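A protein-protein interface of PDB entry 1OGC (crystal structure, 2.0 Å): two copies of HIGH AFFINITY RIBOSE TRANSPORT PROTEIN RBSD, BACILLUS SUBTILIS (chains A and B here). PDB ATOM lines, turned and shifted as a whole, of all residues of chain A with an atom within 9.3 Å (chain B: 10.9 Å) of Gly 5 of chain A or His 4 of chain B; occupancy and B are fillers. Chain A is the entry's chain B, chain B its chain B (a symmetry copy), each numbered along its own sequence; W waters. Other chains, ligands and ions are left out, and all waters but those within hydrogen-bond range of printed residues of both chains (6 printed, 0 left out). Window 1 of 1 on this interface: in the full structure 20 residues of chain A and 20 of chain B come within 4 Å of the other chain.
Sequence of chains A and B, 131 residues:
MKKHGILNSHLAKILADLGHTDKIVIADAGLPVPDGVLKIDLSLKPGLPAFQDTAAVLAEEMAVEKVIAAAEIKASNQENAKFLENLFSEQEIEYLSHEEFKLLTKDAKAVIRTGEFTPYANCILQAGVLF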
ATOM      1  N   LYS A   2     -10.911 -17.463 -18.383  1.00  0.00           N
ATOM      2  CA  LYS A   2     -12.112 -17.600 -19.187  1.00  0.00           C
ATOM      3  C   LYS A   2     -13.235 -16.866 -18.453  1.00  0.00           C
ATOM      4  O   LYS A   2     -13.464 -17.093 -17.266  1.00  0.00           O
ATOM      5  CB  LYS A   2     -12.437 -19.089 -19.339  1.00  0.00           C
ATOM      6  CG  LYS A   2     -13.599 -19.416 -20.247  1.00  0.00           C
ATOM      7  CD  LYS A   2     -13.608 -20.909 -20.582  1.00  0.00           C
ATOM      8  CE  LYS A   2     -13.820 -21.779 -19.351  1.00  0.00           C
ATOM      9  NZ  LYS A   2     -15.259 -21.903 -19.002  1.00  0.00           N
ATOM     10  N   LYS A   3     -13.930 -15.982 -19.160  1.00  0.00           N
ATOM     11  CA  LYS A   3     -15.010 -15.203 -18.558  1.00  0.00           C
ATOM     12  C   LYS A   3     -16.320 -15.939 -18.359  1.00  0.00           C
ATOM     13  O   LYS A   3     -16.963 -15.788 -17.324  1.00  0.00           O
ATOM     14  CB  LYS A   3     -15.297 -13.955 -19.394  1.00  0.00           C
ATOM     15  CG  LYS A   3     -14.278 -12.849 -19.276  1.00  0.00           C
ATOM     16  CD  LYS A   3     -14.699 -11.689 -20.157  1.00  0.00           C
ATOM     17  CE  LYS A   3     -13.719 -10.540 -20.083  1.00  0.00           C
ATOM     18  NZ  LYS A   3     -14.064  -9.497 -21.084  1.00  0.00           N
ATOM     19  N   HIS A   4     -16.721 -16.731 -19.347  1.00  0.00           N
ATOM     20  CA  HIS A   4     -17.991 -17.437 -19.275  1.00  0.00           C
ATOM     21  C   HIS A   4     -17.886 -18.951 -19.318  1.00  0.00           C
ATOM     22  O   HIS A   4     -16.831 -19.511 -19.625  1.00  0.00           O
ATOM     23  CB  HIS A   4     -18.886 -16.977 -20.423  1.00  0.00           C
ATOM     24  CG  HIS A   4     -18.905 -15.493 -20.607  1.00  0.00           C
ATOM     25  ND1 HIS A   4     -18.557 -14.887 -21.795  1.00  0.00           N
ATOM     26  CD2 HIS A   4     -19.210 -14.492 -19.749  1.00  0.00           C
ATOM     27  CE1 HIS A   4     -18.645 -13.576 -21.661  1.00  0.00           C
ATOM     28  NE2 HIS A   4     -19.040 -13.310 -20.428  1.00  0.00           N
ATOM     29  N   GLY A   5     -19.006 -19.604 -19.019  1.00  0.00           N
ATOM     30  CA  GLY A   5     -19.057 -21.054 -19.049  1.00  0.00           C
ATOM     31  C   GLY A   5     -18.713 -21.717 -17.731  1.00  0.00           C
ATOM     32  O   GLY A   5     -18.434 -21.052 -16.736  1.00  0.00           O
ATOM     33  N   ILE A   6     -18.734 -23.043 -17.736  1.00  0.00           N
ATOM     34  CA  ILE A   6     -18.433 -23.829 -16.551  1.00  0.00           C
ATOM     35  C   ILE A   6     -17.004 -23.537 -16.091  1.00  0.00           C
ATOM     36  O   ILE A   6     -16.108 -23.313 -16.911  1.00  0.00           O
ATOM     37  CB  ILE A   6     -18.645 -25.331 -16.860  1.00  0.00           C
ATOM     38  CG1 ILE A   6     -18.759 -26.119 -15.557  1.00  0.00           C
ATOM     39  CG2 ILE A   6     -17.519 -25.853 -17.760  1.00  0.00           C
ATOM     40  CD1 ILE A   6     -19.415 -27.466 -15.741  1.00  0.00           C
ATOM     41  N   LEU A   7     -16.803 -23.512 -14.775  1.00  0.00           N
ATOM     42  CA  LEU A   7     -15.503 -23.212 -14.189  1.00  0.00           C
ATOM     43  C   LEU A   7     -14.464 -24.319 -14.319  1.00  0.00           C
ATOM     44  O   LEU A   7     -13.286 -24.043 -14.516  1.00  0.00           O
ATOM     45  CB  LEU A   7     -15.669 -22.873 -12.699  1.00  0.00           C
ATOM     46  CG  LEU A   7     -14.389 -22.571 -11.906  1.00  0.00           C
ATOM     47  CD1 LEU A   7     -13.742 -21.317 -12.452  1.00  0.00           C
ATOM     48  CD2 LEU A   7     -14.714 -22.401 -10.423  1.00  0.00           C
ATOM     49  N   ASN A   8     -14.896 -25.565 -14.181  1.00  0.00           N
ATOM     50  CA  ASN A   8     -13.980 -26.697 -14.249  1.00  0.00           C
ATOM     51  C   ASN A   8     -13.360 -26.850 -15.636  1.00  0.00           C
ATOM     52  O   ASN A   8     -14.074 -27.017 -16.622  1.00  0.00           O
ATOM     53  CB  ASN A   8     -14.713 -27.975 -13.860  1.00  0.00           C
ATOM     54  CG  ASN A   8     -13.771 -29.142 -13.671  1.00  0.00           C
ATOM     55  OD1 ASN A   8     -13.325 -29.763 -14.640  1.00  0.00           O
ATOM     56  ND2 ASN A   8     -13.442 -29.436 -12.414  1.00  0.00           N
ATOM     57  N   SER A   9     -12.031 -26.798 -15.696  1.00  0.00           N
ATOM     58  CA  SER A   9     -11.315 -26.914 -16.962  1.00  0.00           C
ATOM     59  C   SER A   9     -11.535 -28.260 -17.653  1.00  0.00           C
ATOM     60  O   SER A   9     -11.715 -28.299 -18.868  1.00  0.00           O
ATOM     61  CB  SER A   9      -9.811 -26.646 -16.768  1.00  0.00           C
ATOM     62  OG  SER A   9      -9.224 -27.550 -15.851  1.00  0.00           O
ATOM     63  N   LEU A  11     -14.167 -30.318 -17.396  1.00  0.00           N
ATOM     64  CA  LEU A  11     -15.533 -30.369 -17.895  1.00  0.00           C
ATOM     65  C   LEU A  11     -15.772 -29.422 -19.072  1.00  0.00           C
ATOM     66  O   LEU A  11     -16.553 -29.733 -19.971  1.00  0.00           O
ATOM     67  CB  LEU A  11     -16.531 -30.055 -16.770  1.00  0.00           C
ATOM     68  CG  LEU A  11     -16.667 -31.081 -15.638  1.00  0.00           C
ATOM     69  CD1 LEU A  11     -17.750 -30.627 -14.658  1.00  0.00           C
ATOM     70  CD2 LEU A  11     -17.028 -32.428 -16.219  1.00  0.00           C
ATOM     71  N   ALA A  12     -15.105 -28.272 -19.056  1.00  0.00           N
ATOM     72  CA  ALA A  12     -15.258 -27.292 -20.130  1.00  0.00           C
ATOM     73  C   ALA A  12     -14.798 -27.911 -21.447  1.00  0.00           C
ATOM     74  O   ALA A  12     -15.410 -27.699 -22.490  1.00  0.00           O
ATOM     75  CB  ALA A  12     -14.446 -26.037 -19.823  1.00  0.00           C
ATOM     76  N   LEU A  15     -17.586 -30.332 -22.569  1.00  0.00           N
ATOM     77  CA  LEU A  15     -18.790 -29.645 -23.045  1.00  0.00           C
ATOM     78  C   LEU A  15     -18.521 -29.007 -24.408  1.00  0.00           C
ATOM     79  O   LEU A  15     -19.408 -28.938 -25.258  1.00  0.00           O
ATOM     80  CB  LEU A  15     -19.230 -28.556 -22.056  1.00  0.00           C
ATOM     81  CG  LEU A  15     -19.675 -29.058 -20.682  1.00  0.00           C
ATOM     82  CD1 LEU A  15     -20.129 -27.891 -19.806  1.00  0.00           C
ATOM     83  CD2 LEU A  15     -20.800 -30.055 -20.874  1.00  0.00           C
ATOM     84  N   ALA A  16     -17.292 -28.543 -24.598  1.00  0.00           N
ATOM     85  CA  ALA A  16     -16.890 -27.907 -25.842  1.00  0.00           C
ATOM     86  C   ALA A  16     -17.065 -28.813 -27.059  1.00  0.00           C
ATOM     87  O   ALA A  16     -17.369 -28.330 -28.147  1.00  0.00           O
ATOM     88  CB  ALA A  16     -15.451 -27.449 -25.737  1.00  0.00           C
ATOM     89  N   ALA A  56     -26.910 -29.765 -10.994  1.00  0.00           N
ATOM     90  CA  ALA A  56     -27.410 -28.398 -11.125  1.00  0.00           C
ATOM     91  C   ALA A  56     -26.464 -27.533 -11.957  1.00  0.00           C
ATOM     92  O   ALA A  56     -26.900 -26.774 -12.821  1.00  0.00           O
ATOM     93  CB  ALA A  56     -27.610 -27.780  -9.737  1.00  0.00           C
ATOM     94  N   VAL A  57     -25.166 -27.630 -11.692  1.00  0.00           N
ATOM     95  CA  VAL A  57     -24.206 -26.850 -12.461  1.00  0.00           C
ATOM     96  C   VAL A  57     -24.271 -27.259 -13.934  1.00  0.00           C
ATOM     97  O   VAL A  57     -24.322 -26.409 -14.820  1.00  0.00           O
ATOM     98  CB  VAL A  57     -22.765 -27.053 -11.943  1.00  0.00           C
ATOM     99  CG1 VAL A  57     -21.774 -26.377 -12.884  1.00  0.00           C
ATOM    100  CG2 VAL A  57     -22.630 -26.469 -10.539  1.00  0.00           C
ATOM    101  N   LEU A  58     -24.279 -28.564 -14.193  1.00  0.00           N
ATOM    102  CA  LEU A  58     -24.339 -29.060 -15.564  1.00  0.00           C
ATOM    103  C   LEU A  58     -25.600 -28.615 -16.311  1.00  0.00           C
ATOM    104  O   LEU A  58     -25.526 -28.161 -17.456  1.00  0.00           O
ATOM    105  CB  LEU A  58     -24.237 -30.592 -15.579  1.00  0.00           C
ATOM    106  CG  LEU A  58     -22.832 -31.197 -15.747  1.00  0.00           C
ATOM    107  CD1 LEU A  58     -22.287 -30.819 -17.113  1.00  0.00           C
ATOM    108  CD2 LEU A  58     -21.892 -30.698 -14.668  1.00  0.00           C
ATOM    109  N   ALA A  59     -26.756 -28.736 -15.662  1.00  0.00           N
ATOM    110  CA  ALA A  59     -28.016 -28.346 -16.282  1.00  0.00           C
ATOM    111  C   ALA A  59     -28.001 -26.885 -16.725  1.00  0.00           C
ATOM    112  O   ALA A  59     -28.689 -26.502 -17.671  1.00  0.00           O
ATOM    113  CB  ALA A  59     -29.171 -28.581 -15.314  1.00  0.00           C
ATOM    114  N   GLU A  60     -27.201 -26.076 -16.047  1.00  0.00           N
ATOM    115  CA  GLU A  60     -27.118 -24.658 -16.359  1.00  0.00           C
ATOM    116  C   GLU A  60     -26.078 -24.334 -17.440  1.00  0.00           C
ATOM    117  O   GLU A  60     -26.143 -23.280 -18.069  1.00  0.00           O
ATOM    118  CB  GLU A  60     -26.811 -23.883 -15.071  1.00  0.00           C
ATOM    119  CG  GLU A  60     -27.305 -22.441 -15.068  1.00  0.00           C
ATOM    120  CD  GLU A  60     -26.358 -21.492 -15.772  1.00  0.00           C
ATOM    121  OE1 GLU A  60     -26.773 -20.348 -16.072  1.00  0.00           O
ATOM    122  OE2 GLU A  60     -25.195 -21.886 -16.018  1.00  0.00           O
ATOM    123  N   GLU A  61     -25.138 -25.247 -17.671  1.00  0.00           N
ATOM    124  CA  GLU A  61     -24.084 -25.021 -18.663  1.00  0.00           C
ATOM    125  C   GLU A  61     -24.205 -25.874 -19.921  1.00  0.00           C
ATOM    126  O   GLU A  61     -23.483 -25.666 -20.897  1.00  0.00           O
ATOM    127  CB  GLU A  61     -22.715 -25.280 -18.033  1.00  0.00           C
ATOM    128  CG  GLU A  61     -22.355 -24.360 -16.881  1.00  0.00           C
ATOM    129  CD  GLU A  61     -22.339 -22.899 -17.275  1.00  0.00           C
ATOM    130  OE1 GLU A  61     -22.198 -22.593 -18.481  1.00  0.00           O
ATOM    131  OE2 GLU A  61     -22.455 -22.052 -16.371  1.00  0.00           O
ATOM    132  N   MET A  62     -25.128 -26.825 -19.890  1.00  0.00           N
ATOM    133  CA  MET A  62     -25.344 -27.742 -20.999  1.00  0.00           C
ATOM    134  C   MET A  62     -26.814 -27.797 -21.416  1.00  0.00           C
ATOM    135  O   MET A  62     -27.708 -27.809 -20.570  1.00  0.00           O
ATOM    136  CB  MET A  62     -24.878 -29.136 -20.569  1.00  0.00           C
ATOM    137  CG  MET A  62     -25.111 -30.251 -21.556  1.00  0.00           C
ATOM    138  SD  MET A  62     -24.654 -31.820 -20.785  1.00  0.00           S
ATOM    139  CE  MET A  62     -25.350 -32.983 -21.953  1.00  0.00           C
ATOM    140  N   ALA A  63     -27.059 -27.829 -22.722  1.00  0.00           N
ATOM    141  CA  ALA A  63     -28.418 -27.927 -23.241  1.00  0.00           C
ATOM    142  C   ALA A  63     -28.776 -29.410 -23.219  1.00  0.00           C
ATOM    143  O   ALA A  63     -28.194 -30.214 -23.953  1.00  0.00           O
ATOM    144  CB  ALA A  63     -28.484 -27.388 -24.663  1.00  0.00           C
ATOM    145  N   LEU A 130     -28.774 -25.961 -29.884  1.00  0.00           N
ATOM    146  CA  LEU A 130     -29.166 -24.568 -29.663  1.00  0.00           C
ATOM    147  C   LEU A 130     -29.887 -23.890 -30.828  1.00  0.00           C
ATOM    148  O   LEU A 130     -30.037 -22.669 -30.840  1.00  0.00           O
ATOM    149  CB  LEU A 130     -27.935 -23.733 -29.292  1.00  0.00           C
ATOM    150  CG  LEU A 130     -27.171 -24.126 -28.025  1.00  0.00           C
ATOM    151  CD1 LEU A 130     -25.911 -23.286 -27.908  1.00  0.00           C
ATOM    152  CD2 LEU A 130     -28.065 -23.944 -26.802  1.00  0.00           C
ATOM    153  N   MET B   1     -25.268 -29.617 -26.225  1.00  0.00           N
ATOM    154  CA  MET B   1     -24.341 -28.515 -26.607  1.00  0.00           C
ATOM    155  C   MET B   1     -24.040 -27.603 -25.431  1.00  0.00           C
ATOM    156  O   MET B   1     -24.832 -27.479 -24.500  1.00  0.00           O
ATOM    157  CB  MET B   1     -24.934 -27.666 -27.735  1.00  0.00           C
ATOM    158  CG  MET B   1     -24.908 -28.314 -29.110  1.00  0.00           C
ATOM    159  SD  MET B   1     -25.513 -27.181 -30.388  1.00  0.00           S
ATOM    160  CE  MET B   1     -24.149 -26.029 -30.511  1.00  0.00           C
ATOM    161  N   LYS B   2     -22.884 -26.959 -25.498  1.00  0.00           N
ATOM    162  CA  LYS B   2     -22.441 -26.032 -24.472  1.00  0.00           C
ATOM    163  C   LYS B   2     -23.257 -24.749 -24.636  1.00  0.00           C
ATOM    164  O   LYS B   2     -23.343 -24.194 -25.730  1.00  0.00           O
ATOM    165  CB  LYS B   2     -20.946 -25.762 -24.663  1.00  0.00           C
ATOM    166  CG  LYS B   2     -20.296 -24.902 -23.605  1.00  0.00           C
ATOM    167  CD  LYS B   2     -18.772 -24.985 -23.715  1.00  0.00           C
ATOM    168  CE  LYS B   2     -18.254 -24.434 -25.036  1.00  0.00           C
ATOM    169  NZ  LYS B   2     -18.117 -22.955 -25.002  1.00  0.00           N
ATOM    170  N   LYS B   3     -23.859 -24.283 -23.548  1.00  0.00           N
ATOM    171  CA  LYS B   3     -24.685 -23.078 -23.589  1.00  0.00           C
ATOM    172  C   LYS B   3     -23.930 -21.764 -23.625  1.00  0.00           C
ATOM    173  O   LYS B   3     -24.305 -20.855 -24.362  1.00  0.00           O
ATOM    174  CB  LYS B   3     -25.633 -23.039 -22.391  1.00  0.00           C
ATOM    175  CG  LYS B   3     -26.806 -23.986 -22.463  1.00  0.00           C
ATOM    176  CD  LYS B   3     -27.648 -23.832 -21.212  1.00  0.00           C
ATOM    177  CE  LYS B   3     -28.847 -24.753 -21.222  1.00  0.00           C
ATOM    178  NZ  LYS B   3     -29.550 -24.705 -19.912  1.00  0.00           N
ATOM    179  N   HIS B   4     -22.871 -21.657 -22.831  1.00  0.00           N
ATOM    180  CA  HIS B   4     -22.114 -20.417 -22.752  1.00  0.00           C
ATOM    181  C   HIS B   4     -20.658 -20.528 -23.168  1.00  0.00           C
ATOM    182  O   HIS B   4     -20.120 -21.626 -23.329  1.00  0.00           O
ATOM    183  CB  HIS B   4     -22.175 -19.882 -21.323  1.00  0.00           C
ATOM    184  CG  HIS B   4     -23.547 -19.918 -20.731  1.00  0.00           C
ATOM    185  ND1 HIS B   4     -23.834 -20.588 -19.561  1.00  0.00           N
ATOM    186  CD2 HIS B   4     -24.716 -19.385 -21.156  1.00  0.00           C
ATOM    187  CE1 HIS B   4     -25.122 -20.467 -19.290  1.00  0.00           C
ATOM    188  NE2 HIS B   4     -25.680 -19.741 -20.243  1.00  0.00           N
ATOM    189  N   GLY B   5     -20.025 -19.368 -23.323  1.00  0.00           N
ATOM    190  CA  GLY B   5     -18.622 -19.326 -23.691  1.00  0.00           C
ATOM    191  C   GLY B   5     -18.370 -19.283 -25.184  1.00  0.00           C
ATOM    192  O   GLY B   5     -19.299 -19.271 -25.988  1.00  0.00           O
ATOM    193  N   ILE B   6     -17.094 -19.263 -25.548  1.00  0.00           N
ATOM    194  CA  ILE B   6     -16.684 -19.216 -26.942  1.00  0.00           C
ATOM    195  C   ILE B   6     -17.201 -20.458 -27.669  1.00  0.00           C
ATOM    196  O   ILE B   6     -17.264 -21.549 -27.094  1.00  0.00           O
ATOM    197  CB  ILE B   6     -15.143 -19.097 -27.023  1.00  0.00           C
ATOM    198  CG1 ILE B   6     -14.731 -18.621 -28.413  1.00  0.00           C
ATOM    199  CG2 ILE B   6     -14.486 -20.431 -26.646  1.00  0.00           C
ATOM    200  CD1 ILE B   6     -13.338 -18.041 -28.446  1.00  0.00           C
ATOM    201  N   LEU B   7     -17.597 -20.280 -28.928  1.00  0.00           N
ATOM    202  CA  LEU B   7     -18.145 -21.362 -29.735  1.00  0.00           C
ATOM    203  C   LEU B   7     -17.129 -22.395 -30.209  1.00  0.00           C
ATOM    204  O   LEU B   7     -17.433 -23.581 -30.269  1.00  0.00           O
ATOM    205  CB  LEU B   7     -18.861 -20.784 -30.966  1.00  0.00           C
ATOM    206  CG  LEU B   7     -19.466 -21.788 -31.958  1.00  0.00           C
ATOM    207  CD1 LEU B   7     -20.572 -22.565 -31.277  1.00  0.00           C
ATOM    208  CD2 LEU B   7     -20.005 -21.059 -33.186  1.00  0.00           C
ATOM    209  N   ASN B   8     -15.938 -21.939 -30.570  1.00  0.00           N
ATOM    210  CA  ASN B   8     -14.904 -22.836 -31.075  1.00  0.00           C
ATOM    211  C   ASN B   8     -14.430 -23.822 -30.009  1.00  0.00           C
ATOM    212  O   ASN B   8     -13.948 -23.414 -28.955  1.00  0.00           O
ATOM    213  CB  ASN B   8     -13.726 -22.022 -31.595  1.00  0.00           C
ATOM    214  CG  ASN B   8     -12.731 -22.870 -32.353  1.00  0.00           C
ATOM    215  OD1 ASN B   8     -11.908 -23.570 -31.757  1.00  0.00           O
ATOM    216  ND2 ASN B   8     -12.815 -22.831 -33.681  1.00  0.00           N
ATOM    217  N   SER B   9     -14.568 -25.114 -30.299  1.00  0.00           N
ATOM    218  CA  SER B   9     -14.170 -26.157 -29.360  1.00  0.00           C
ATOM    219  C   SER B   9     -12.674 -26.139 -29.045  1.00  0.00           C
ATOM    220  O   SER B   9     -12.294 -26.309 -27.888  1.00  0.00           O
ATOM    221  CB  SER B   9     -14.597 -27.546 -29.872  1.00  0.00           C
ATOM    222  OG  SER B   9     -14.024 -27.849 -31.129  1.00  0.00           O
ATOM    223  N   LEU B  11     -10.564 -23.539 -29.148  1.00  0.00           N
ATOM    224  CA  LEU B  11     -10.273 -22.368 -28.333  1.00  0.00           C
ATOM    225  C   LEU B  11     -10.844 -22.473 -26.919  1.00  0.00           C
ATOM    226  O   LEU B  11     -10.240 -21.976 -25.967  1.00  0.00           O
ATOM    227  CB  LEU B  11     -10.800 -21.094 -29.011  1.00  0.00           C
ATOM    228  CG  LEU B  11     -10.112 -20.643 -30.304  1.00  0.00           C
ATOM    229  CD1 LEU B  11     -10.728 -19.329 -30.785  1.00  0.00           C
ATOM    230  CD2 LEU B  11      -8.634 -20.459 -30.051  1.00  0.00           C
ATOM    231  N   ALA B  12     -12.003 -23.109 -26.790  1.00  0.00           N
ATOM    232  CA  ALA B  12     -12.640 -23.267 -25.483  1.00  0.00           C
ATOM    233  C   ALA B  12     -11.727 -24.079 -24.570  1.00  0.00           C
ATOM    234  O   ALA B  12     -11.599 -23.786 -23.385  1.00  0.00           O
ATOM    235  CB  ALA B  12     -13.992 -23.961 -25.632  1.00  0.00           C
ATOM    236  N   LYS B  13     -11.080 -25.091 -25.134  1.00  0.00           N
ATOM    237  CA  LYS B  13     -10.168 -25.937 -24.368  1.00  0.00           C
ATOM    238  C   LYS B  13      -8.960 -25.145 -23.875  1.00  0.00           C
ATOM    239  O   LYS B  13      -8.484 -25.346 -22.760  1.00  0.00           O
ATOM    240  CB  LYS B  13      -9.721 -27.119 -25.224  1.00  0.00           C
ATOM    241  CG  LYS B  13     -10.866 -28.043 -25.582  1.00  0.00           C
ATOM    242  CD  LYS B  13     -10.443 -29.155 -26.523  1.00  0.00           C
ATOM    243  CE  LYS B  13     -11.604 -30.090 -26.786  1.00  0.00           C
ATOM    244  NZ  LYS B  13     -11.260 -31.107 -27.800  1.00  0.00           N
ATOM    245  N   LEU B  15      -8.881 -21.716 -23.465  1.00  0.00           N
ATOM    246  CA  LEU B  15      -9.317 -20.696 -22.507  1.00  0.00           C
ATOM    247  C   LEU B  15      -9.582 -21.339 -21.145  1.00  0.00           C
ATOM    248  O   LEU B  15      -9.349 -20.728 -20.103  1.00  0.00           O
ATOM    249  CB  LEU B  15     -10.596 -19.997 -22.991  1.00  0.00           C
ATOM    250  CG  LEU B  15     -10.451 -19.182 -24.277  1.00  0.00           C
ATOM    251  CD1 LEU B  15     -11.773 -18.501 -24.632  1.00  0.00           C
ATOM    252  CD2 LEU B  15      -9.355 -18.155 -24.076  1.00  0.00           C
ATOM    253  N   ALA B  16     -10.071 -22.573 -21.172  1.00  0.00           N
ATOM    254  CA  ALA B  16     -10.377 -23.310 -19.957  1.00  0.00           C
ATOM    255  C   ALA B  16      -9.163 -23.484 -19.045  1.00  0.00           C
ATOM    256  O   ALA B  16      -9.309 -23.500 -17.825  1.00  0.00           O
ATOM    257  CB  ALA B  16     -10.956 -24.661 -20.315  1.00  0.00           C
ATOM    258  N   VAL B  57     -13.827 -11.381 -30.662  1.00  0.00           N
ATOM    259  CA  VAL B  57     -14.442 -12.520 -29.995  1.00  0.00           C
ATOM    260  C   VAL B  57     -13.645 -12.873 -28.736  1.00  0.00           C
ATOM    261  O   VAL B  57     -14.218 -13.075 -27.667  1.00  0.00           O
ATOM    262  CB  VAL B  57     -14.501 -13.756 -30.918  1.00  0.00           C
ATOM    263  CG1 VAL B  57     -14.972 -14.973 -30.130  1.00  0.00           C
ATOM    264  CG2 VAL B  57     -15.451 -13.491 -32.082  1.00  0.00           C
ATOM    265  N   GLU B  60     -13.980 -10.659 -25.664  1.00  0.00           N
ATOM    266  CA  GLU B  60     -15.262 -10.828 -25.000  1.00  0.00           C
ATOM    267  C   GLU B  60     -15.361 -12.131 -24.195  1.00  0.00           C
ATOM    268  O   GLU B  60     -16.197 -12.248 -23.302  1.00  0.00           O
ATOM    269  CB  GLU B  60     -16.379 -10.761 -26.050  1.00  0.00           C
ATOM    270  CG  GLU B  60     -17.724 -10.287 -25.513  1.00  0.00           C
ATOM    271  CD  GLU B  60     -18.518 -11.396 -24.853  1.00  0.00           C
ATOM    272  OE1 GLU B  60     -19.502 -11.084 -24.142  1.00  0.00           O
ATOM    273  OE2 GLU B  60     -18.164 -12.580 -25.053  1.00  0.00           O
ATOM    274  N   GLU B  61     -14.496 -13.097 -24.494  1.00  0.00           N
ATOM    275  CA  GLU B  61     -14.527 -14.388 -23.803  1.00  0.00           C
ATOM    276  C   GLU B  61     -13.358 -14.626 -22.853  1.00  0.00           C
ATOM    277  O   GLU B  61     -13.350 -15.594 -22.091  1.00  0.00           O
ATOM    278  CB  GLU B  61     -14.556 -15.524 -24.826  1.00  0.00           C
ATOM    279  CG  GLU B  61     -15.779 -15.546 -25.725  1.00  0.00           C
ATOM    280  CD  GLU B  61     -17.075 -15.674 -24.955  1.00  0.00           C
ATOM    281  OE1 GLU B  61     -17.053 -16.150 -23.797  1.00  0.00           O
ATOM    282  OE2 GLU B  61     -18.124 -15.309 -25.517  1.00  0.00           O
ATOM    283  N   MET B  62     -12.382 -13.729 -22.899  1.00  0.00           N
ATOM    284  CA  MET B  62     -11.186 -13.834 -22.078  1.00  0.00           C
ATOM    285  C   MET B  62     -10.904 -12.542 -21.312  1.00  0.00           C
ATOM    286  O   MET B  62     -11.052 -11.444 -21.852  1.00  0.00           O
ATOM    287  CB  MET B  62     -10.001 -14.158 -22.994  1.00  0.00           C
ATOM    288  CG  MET B  62      -8.645 -14.211 -22.336  1.00  0.00           C
ATOM    289  SD  MET B  62      -7.384 -14.430 -23.612  1.00  0.00           S
ATOM    290  CE  MET B  62      -5.898 -14.090 -22.677  1.00  0.00           C
ATOM    291  N   LEU B 130     -10.219 -13.050 -12.470  1.00  0.00           N
ATOM    292  CA  LEU B 130     -11.585 -12.614 -12.174  1.00  0.00           C
ATOM    293  C   LEU B 130     -11.864 -12.251 -10.716  1.00  0.00           C
ATOM    294  O   LEU B 130     -13.020 -12.112 -10.320  1.00  0.00           O
ATOM    295  CB  LEU B 130     -12.583 -13.691 -12.614  1.00  0.00           C
ATOM    296  CG  LEU B 130     -12.608 -14.067 -14.098  1.00  0.00           C
ATOM    297  CD1 LEU B 130     -13.545 -15.244 -14.310  1.00  0.00           C
ATOM    298  CD2 LEU B 130     -13.044 -12.864 -14.930  1.00  0.00           C
HETATM  299  O   HOH W   1     -20.756 -27.885 -27.594  1.00  0.00           O
HETATM  300  O   HOH W   2     -21.866 -23.463 -21.005  1.00  0.00           O
HETATM  301  O   HOH W   3     -17.591 -25.447 -28.113  1.00  0.00           O
HETATM  302  O   HOH W   4      -9.620 -20.095 -17.291  1.00  0.00           O
HETATM  303  O   HOH W   5     -12.067 -23.281 -16.984  1.00  0.00           O
HETATM  304  O   HOH W   6     -15.562 -17.178 -21.809  1.00  0.00           O
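Lys 2 of chain A touches Ala 16 of chain B, and with the chains exchanged Ala 16 of chain A touches Lys 2 of chain B.
Positions printed for both chains: 2, 3, 4, 5, 6, 7, 8, 9, 11, 12, 15, 16, 57, 60, 61, 62 and 130.
Of the 19 printed residues of chain B, 13 touch a printed residue of chain A.
Hydrophobic or aromatic side chains of chain B that line the printed part of chain A: Met 1, His 4, Ala 12, Leu 15, Ala 16 and Leu 130.
Of the 21 printed residues of chain A, 14 touch a printed residue of chain B.
Hydrophobic or aromatic side chains of chain A that line the printed part of chain B: His 4, Ala 12, Leu 15, Ala 16, Ala 63 and Leu 130.
Along chain A the printed residues that touch a printed residue of chain B span positions 2 to 130.
Among the printed residues, 29 pairs touch across the chains.
Among the printed residues, no Asp or Glu carboxylate lies within 4 Å of a Lys or Arg side-chain nitrogen of the other chain.
Lys 3 of chain A touches Met 62 of chain B.
His 4 of chain A touches Glu 60 of chain B.
O of Leu 15 of chain A touches CB of Lys 2 of chain B (3.6 Å).
Lys 2 of chain B touches Ala 16 of chain A.
Glu 60 of chain A touches Lys 3 of chain B.
Ala 63 of chain A touches Lys 3 of chain B (CA to CE, 3.8 Å).
Gly 5 of chain A touches just one residue of chain B: His 4.
Glu 60 of chain A touches just these residues of chain B: Lys 3 and His 4.
Of the printed residues of chain B, Ala 16 of chain A touches Lys 2 (3.8 Å), Ser 9 (3.4 Å) and Ala 12 (3.8 Å).
Printed residues of chain B within 4 Å of Ala 12 of chain A: Ala 16 (3.8 Å).
Of the printed residues of chain B, Leu 15 of chain A touches Lys 2 (3.6 Å).
The nearest residue of chain A that does not touch His 4 of chain B is His 4 of chain A (4.5 Å).
NZ of Lys 2 of chain A sits at hydrogen-bond distance from O of Ile 6 of chain A, at 2.7 Å.
The side-chain amino group of Lys 2 of chain B is in hydrogen-bond range of the backbone carbonyl oxygen of Ile 6 of chain B, 2.7 Å away.
Water W3 lies within hydrogen-bond range of O of Leu 7 of chain B and O of Ala 16 of chain A.
The backbone carbonyl oxygen (O) of Glu 61 of chain A sits at hydrogen-bond distance from the backbone NH (N) of Lys 3 of chain B, 3.0 Å away.
The side-chain amino group (NZ) of Lys 3 of chain B sits at hydrogen-bond distance from the backbone carbonyl oxygen (O) of Ala 59 of chain A, 3.0 Å away.
The side-chain carboxylate of Glu 61 of chain A sits at hydrogen-bond distance from a ring nitrogen (ND1) of His 4 of chain B (2.8 Å).
A ring nitrogen (ND1) of His 4 of chain A lies within hydrogen-bond range of the side-chain carboxylate (OE1) of Glu 61 of chain B (2.8 Å).
N of Ala 63 of chain A sits at hydrogen-bond distance from O of Met 1 of chain B, 2.9 Å away.
The backbone NH of Leu 130 of chain A is in hydrogen-bond range of the side-chain sulfur of Met 1 of chain B (3.5 Å).
The backbone NH (N) of Lys 3 of chain A sits at hydrogen-bond distance from the backbone carbonyl oxygen (O) of Glu 61 of chain B (3.0 Å).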
